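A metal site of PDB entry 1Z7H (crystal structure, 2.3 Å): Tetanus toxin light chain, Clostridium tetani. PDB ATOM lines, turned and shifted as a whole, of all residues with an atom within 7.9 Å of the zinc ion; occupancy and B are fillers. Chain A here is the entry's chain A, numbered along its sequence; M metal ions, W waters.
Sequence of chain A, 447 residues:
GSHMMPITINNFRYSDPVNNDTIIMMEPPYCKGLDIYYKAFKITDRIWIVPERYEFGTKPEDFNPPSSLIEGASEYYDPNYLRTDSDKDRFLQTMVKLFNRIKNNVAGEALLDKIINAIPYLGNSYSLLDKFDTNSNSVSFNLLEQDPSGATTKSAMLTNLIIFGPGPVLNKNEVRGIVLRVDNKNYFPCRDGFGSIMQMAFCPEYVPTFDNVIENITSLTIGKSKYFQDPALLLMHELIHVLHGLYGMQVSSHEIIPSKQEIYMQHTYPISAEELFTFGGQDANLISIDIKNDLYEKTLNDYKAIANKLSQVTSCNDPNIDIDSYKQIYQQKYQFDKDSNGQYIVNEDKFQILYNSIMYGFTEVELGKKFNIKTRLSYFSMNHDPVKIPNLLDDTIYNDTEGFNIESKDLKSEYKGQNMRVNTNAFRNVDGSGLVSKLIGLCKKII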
ATOM      1  N   ASN A 173      27.068  -4.919  11.063  1.00  0.00           N
ATOM      2  CA  ASN A 173      26.802  -4.156   9.851  1.00  0.00           C
ATOM      3  C   ASN A 173      25.300  -3.994   9.651  1.00  0.00           C
ATOM      4  O   ASN A 173      24.531  -4.918   9.901  1.00  0.00           O
ATOM      5  CB  ASN A 173      27.434  -4.850   8.646  1.00  0.00           C
ATOM      6  CG  ASN A 173      28.924  -5.044   8.808  1.00  0.00           C
ATOM      7  OD1 ASN A 173      29.651  -4.137   9.213  1.00  0.00           O
ATOM      8  ND2 ASN A 173      29.394  -6.242   8.474  1.00  0.00           N
ATOM      9  N   GLU A 174      24.891  -2.821   9.194  1.00  0.00           N
ATOM     10  CA  GLU A 174      23.477  -2.572   8.996  1.00  0.00           C
ATOM     11  C   GLU A 174      23.204  -1.587   7.872  1.00  0.00           C
ATOM     12  O   GLU A 174      24.017  -0.713   7.568  1.00  0.00           O
ATOM     13  CB  GLU A 174      22.877  -2.041  10.313  1.00  0.00           C
ATOM     14  CG  GLU A 174      21.421  -2.400  10.539  1.00  0.00           C
ATOM     15  CD  GLU A 174      20.902  -1.901  11.880  1.00  0.00           C
ATOM     16  OE1 GLU A 174      21.604  -2.043  12.893  1.00  0.00           O
ATOM     17  OE2 GLU A 174      19.765  -1.368  11.911  1.00  0.00           O
ATOM     18  N   VAL A 175      22.046  -1.735   7.245  1.00  0.00           N
ATOM     19  CA  VAL A 175      21.638  -0.854   6.158  1.00  0.00           C
ATOM     20  C   VAL A 175      20.230  -0.349   6.434  1.00  0.00           C
ATOM     21  O   VAL A 175      19.329  -1.124   6.781  1.00  0.00           O
ATOM     22  CB  VAL A 175      21.646  -1.601   4.805  1.00  0.00           C
ATOM     23  CG1 VAL A 175      20.924  -0.782   3.757  1.00  0.00           C
ATOM     24  CG2 VAL A 175      23.075  -1.879   4.365  1.00  0.00           C
ATOM     25  N   LEU A 234      30.661  -9.755   3.213  1.00  0.00           N
ATOM     26  CA  LEU A 234      29.783  -9.117   4.190  1.00  0.00           C
ATOM     27  C   LEU A 234      29.318  -7.799   3.570  1.00  0.00           C
ATOM     28  O   LEU A 234      28.159  -7.418   3.686  1.00  0.00           O
ATOM     29  CB  LEU A 234      30.527  -8.858   5.510  1.00  0.00           C
ATOM     30  CG  LEU A 234      31.060 -10.111   6.218  1.00  0.00           C
ATOM     31  CD1 LEU A 234      31.977  -9.673   7.342  1.00  0.00           C
ATOM     32  CD2 LEU A 234      29.910 -10.967   6.753  1.00  0.00           C
ATOM     33  N   HIS A 237      26.801  -8.418   0.989  1.00  0.00           N
ATOM     34  CA  HIS A 237      25.581  -8.795   1.692  1.00  0.00           C
ATOM     35  C   HIS A 237      24.787  -7.503   1.972  1.00  0.00           C
ATOM     36  O   HIS A 237      23.604  -7.399   1.650  1.00  0.00           O
ATOM     37  CB  HIS A 237      25.942  -9.473   3.007  1.00  0.00           C
ATOM     38  CG  HIS A 237      24.751  -9.783   3.865  1.00  0.00           C
ATOM     39  ND1 HIS A 237      24.117 -11.002   3.835  1.00  0.00           N
ATOM     40  CD2 HIS A 237      24.075  -9.029   4.761  1.00  0.00           C
ATOM     41  CE1 HIS A 237      23.104 -10.995   4.684  1.00  0.00           C
ATOM     42  NE2 HIS A 237      23.056  -9.803   5.255  1.00  0.00           N
ATOM     43  N   GLU A 238      25.469  -6.515   2.558  1.00  0.00           N
ATOM     44  CA  GLU A 238      24.822  -5.242   2.868  1.00  0.00           C
ATOM     45  C   GLU A 238      24.422  -4.525   1.586  1.00  0.00           C
ATOM     46  O   GLU A 238      23.339  -3.922   1.506  1.00  0.00           O
ATOM     47  CB  GLU A 238      25.755  -4.355   3.698  1.00  0.00           C
ATOM     48  CG  GLU A 238      26.118  -4.910   5.072  1.00  0.00           C
ATOM     49  CD  GLU A 238      24.907  -5.468   5.835  1.00  0.00           C
ATOM     50  OE1 GLU A 238      23.890  -4.767   5.971  1.00  0.00           O
ATOM     51  OE2 GLU A 238      24.972  -6.622   6.307  1.00  0.00           O
ATOM     52  N   ILE A 240      23.364  -5.790  -1.013  1.00  0.00           N
ATOM     53  CA  ILE A 240      22.137  -6.394  -1.516  1.00  0.00           C
ATOM     54  C   ILE A 240      20.948  -5.704  -0.831  1.00  0.00           C
ATOM     55  O   ILE A 240      19.943  -5.379  -1.471  1.00  0.00           O
ATOM     56  CB  ILE A 240      22.128  -7.944  -1.294  1.00  0.00           C
ATOM     57  CG1 ILE A 240      23.183  -8.579  -2.211  1.00  0.00           C
ATOM     58  CG2 ILE A 240      20.740  -8.549  -1.599  1.00  0.00           C
ATOM     59  CD1 ILE A 240      23.374 -10.083  -2.011  1.00  0.00           C
ATOM     60  N   HIS A 241      21.090  -5.454   0.477  1.00  0.00           N
ATOM     61  CA  HIS A 241      20.048  -4.744   1.211  1.00  0.00           C
ATOM     62  C   HIS A 241      19.864  -3.373   0.610  1.00  0.00           C
ATOM     63  O   HIS A 241      18.753  -2.854   0.566  1.00  0.00           O
ATOM     64  CB  HIS A 241      20.417  -4.602   2.681  1.00  0.00           C
ATOM     65  CG  HIS A 241      20.165  -5.831   3.476  1.00  0.00           C
ATOM     66  ND1 HIS A 241      19.026  -6.590   3.333  1.00  0.00           N
ATOM     67  CD2 HIS A 241      20.937  -6.472   4.395  1.00  0.00           C
ATOM     68  CE1 HIS A 241      19.100  -7.647   4.112  1.00  0.00           C
ATOM     69  NE2 HIS A 241      20.247  -7.600   4.773  1.00  0.00           N
ATOM     70  N   SER A 272      13.765 -11.580   9.921  1.00  0.00           N
ATOM     71  CA  SER A 272      13.081 -10.768   8.916  1.00  0.00           C
ATOM     72  C   SER A 272      13.206 -11.420   7.545  1.00  0.00           C
ATOM     73  O   SER A 272      14.243 -11.984   7.211  1.00  0.00           O
ATOM     74  CB  SER A 272      13.683  -9.360   8.868  1.00  0.00           C
ATOM     75  OG  SER A 272      15.033  -9.400   8.441  1.00  0.00           O
ATOM     76  N   GLU A 274      13.505  -9.993   4.846  1.00  0.00           N
ATOM     77  CA  GLU A 274      14.556  -9.242   4.153  1.00  0.00           C
ATOM     78  C   GLU A 274      15.876 -10.007   4.276  1.00  0.00           C
ATOM     79  O   GLU A 274      16.619 -10.138   3.311  1.00  0.00           O
ATOM     80  CB  GLU A 274      14.678  -7.839   4.771  1.00  0.00           C
ATOM     81  CG  GLU A 274      15.836  -6.978   4.278  1.00  0.00           C
ATOM     82  CD  GLU A 274      15.672  -6.468   2.847  1.00  0.00           C
ATOM     83  OE1 GLU A 274      14.521  -6.290   2.403  1.00  0.00           O
ATOM     84  OE2 GLU A 274      16.699  -6.229   2.181  1.00  0.00           O
ATOM     85  N   GLU A 275      16.154 -10.514   5.474  1.00  0.00           N
ATOM     86  CA  GLU A 275      17.389 -11.248   5.675  1.00  0.00           C
ATOM     87  C   GLU A 275      17.421 -12.571   4.911  1.00  0.00           C
ATOM     88  O   GLU A 275      18.438 -12.922   4.312  1.00  0.00           O
ATOM     89  CB  GLU A 275      17.616 -11.522   7.164  1.00  0.00           C
ATOM     90  CG  GLU A 275      17.954 -10.282   8.002  1.00  0.00           C
ATOM     91  CD  GLU A 275      19.166  -9.510   7.499  1.00  0.00           C
ATOM     92  OE1 GLU A 275      20.006 -10.101   6.779  1.00  0.00           O
ATOM     93  OE2 GLU A 275      19.285  -8.308   7.841  1.00  0.00           O
ATOM     94  N   LEU A 276      16.324 -13.316   4.932  1.00  0.00           N
ATOM     95  CA  LEU A 276      16.261 -14.595   4.232  1.00  0.00           C
ATOM     96  C   LEU A 276      16.402 -14.431   2.718  1.00  0.00           C
ATOM     97  O   LEU A 276      17.087 -15.219   2.077  1.00  0.00           O
ATOM     98  CB  LEU A 276      14.960 -15.321   4.595  1.00  0.00           C
ATOM     99  CG  LEU A 276      14.993 -16.216   5.851  1.00  0.00           C
ATOM    100  CD1 LEU A 276      15.863 -15.608   6.945  1.00  0.00           C
ATOM    101  CD2 LEU A 276      13.576 -16.439   6.338  1.00  0.00           C
ATOM    102  N   THR A 278      17.899 -11.941   1.171  1.00  0.00           N
ATOM    103  CA  THR A 278      19.279 -11.510   0.966  1.00  0.00           C
ATOM    104  C   THR A 278      20.289 -12.643   1.048  1.00  0.00           C
ATOM    105  O   THR A 278      21.200 -12.738   0.236  1.00  0.00           O
ATOM    106  CB  THR A 278      19.645 -10.403   1.978  1.00  0.00           C
ATOM    107  OG1 THR A 278      18.788  -9.274   1.773  1.00  0.00           O
ATOM    108  CG2 THR A 278      21.101  -9.967   1.788  1.00  0.00           C
ATOM    109  N   PHE A 279      20.103 -13.518   2.034  1.00  0.00           N
ATOM    110  CA  PHE A 279      21.012 -14.654   2.194  1.00  0.00           C
ATOM    111  C   PHE A 279      20.839 -15.611   1.013  1.00  0.00           C
ATOM    112  O   PHE A 279      21.816 -16.108   0.452  1.00  0.00           O
ATOM    113  CB  PHE A 279      20.712 -15.390   3.499  1.00  0.00           C
ATOM    114  CG  PHE A 279      21.677 -16.512   3.784  1.00  0.00           C
ATOM    115  CD1 PHE A 279      22.991 -16.232   4.166  1.00  0.00           C
ATOM    116  CD2 PHE A 279      21.276 -17.837   3.662  1.00  0.00           C
ATOM    117  CE1 PHE A 279      23.886 -17.253   4.419  1.00  0.00           C
ATOM    118  CE2 PHE A 279      22.169 -18.865   3.909  1.00  0.00           C
ATOM    119  CZ  PHE A 279      23.475 -18.576   4.298  1.00  0.00           C
ATOM    120  N   GLU A 364      23.811 -13.755  -0.941  1.00  0.00           N
ATOM    121  CA  GLU A 364      25.099 -14.044  -0.309  1.00  0.00           C
ATOM    122  C   GLU A 364      25.610 -15.403  -0.773  1.00  0.00           C
ATOM    123  O   GLU A 364      26.777 -15.545  -1.146  1.00  0.00           O
ATOM    124  CB  GLU A 364      24.957 -14.048   1.217  1.00  0.00           C
ATOM    125  CG  GLU A 364      26.296 -14.087   1.944  1.00  0.00           C
ATOM    126  CD  GLU A 364      26.162 -14.151   3.461  1.00  0.00           C
ATOM    127  OE1 GLU A 364      25.319 -13.415   4.015  1.00  0.00           O
ATOM    128  OE2 GLU A 364      26.920 -14.922   4.085  1.00  0.00           O
ATOM    129  N   ARG A 376      28.279 -20.110   5.127  1.00  0.00           N
ATOM    130  CA  ARG A 376      27.619 -21.055   6.009  1.00  0.00           C
ATOM    131  C   ARG A 376      26.369 -21.607   5.331  1.00  0.00           C
ATOM    132  O   ARG A 376      25.901 -21.050   4.346  1.00  0.00           O
ATOM    133  CB  ARG A 376      27.291 -20.405   7.347  1.00  0.00           C
ATOM    134  CG  ARG A 376      26.404 -19.174   7.275  1.00  0.00           C
ATOM    135  CD  ARG A 376      26.339 -18.525   8.641  1.00  0.00           C
ATOM    136  NE  ARG A 376      25.280 -17.523   8.763  1.00  0.00           N
ATOM    137  CZ  ARG A 376      25.280 -16.333   8.152  1.00  0.00           C
ATOM    138  NH1 ARG A 376      26.295 -15.986   7.368  1.00  0.00           N
ATOM    139  NH2 ARG A 376      24.279 -15.489   8.350  1.00  0.00           N
ATOM    140  N   TYR A 379      21.320 -18.869   7.254  1.00  0.00           N
ATOM    141  CA  TYR A 379      21.415 -17.613   7.986  1.00  0.00           C
ATOM    142  C   TYR A 379      21.283 -17.932   9.477  1.00  0.00           C
ATOM    143  O   TYR A 379      21.717 -17.153  10.327  1.00  0.00           O
ATOM    144  CB  TYR A 379      20.299 -16.668   7.552  1.00  0.00           C
ATOM    145  CG  TYR A 379      20.347 -15.319   8.218  1.00  0.00           C
ATOM    146  CD1 TYR A 379      21.363 -14.410   7.922  1.00  0.00           C
ATOM    147  CD2 TYR A 379      19.405 -14.962   9.178  1.00  0.00           C
ATOM    148  CE1 TYR A 379      21.439 -13.170   8.565  1.00  0.00           C
ATOM    149  CE2 TYR A 379      19.472 -13.726   9.830  1.00  0.00           C
ATOM    150  CZ  TYR A 379      20.493 -12.841   9.528  1.00  0.00           C
ATOM    151  OH  TYR A 379      20.565 -11.628  10.174  1.00  0.00           O
HETATM  152 ZN    ZN M   1      21.513  -8.633   6.374  1.00  0.00          ZN
HETATM  153  O   HOH W   1      22.457  -6.976   7.536  1.00  0.00           O
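OE2 of Glu 274 sits at hydrogen-bond distance from ND1 of His 241 (2.6 Å).
N of Glu 275 sits close to OG of Ser 272, 3.4 Å away.
A ring nitrogen (ND1) of His 241 sits close to the side-chain hydroxyl of Thr 278, at 3.1 Å.
ND1 of His 237 sits at hydrogen-bond distance from OE1 of Glu 364.
The zinc ion is bound by the side-chain carboxylate of Glu 275, water W1, a ring nitrogen (NE2) of His 237 and a ring nitrogen (NE2) of His 241.
Slightly farther from the zinc ion lies OE2 of Glu 275 (2.7 Å).
Water W1 lies within hydrogen-bond range of OE2 of Glu 238 and OE2 of Glu 275.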
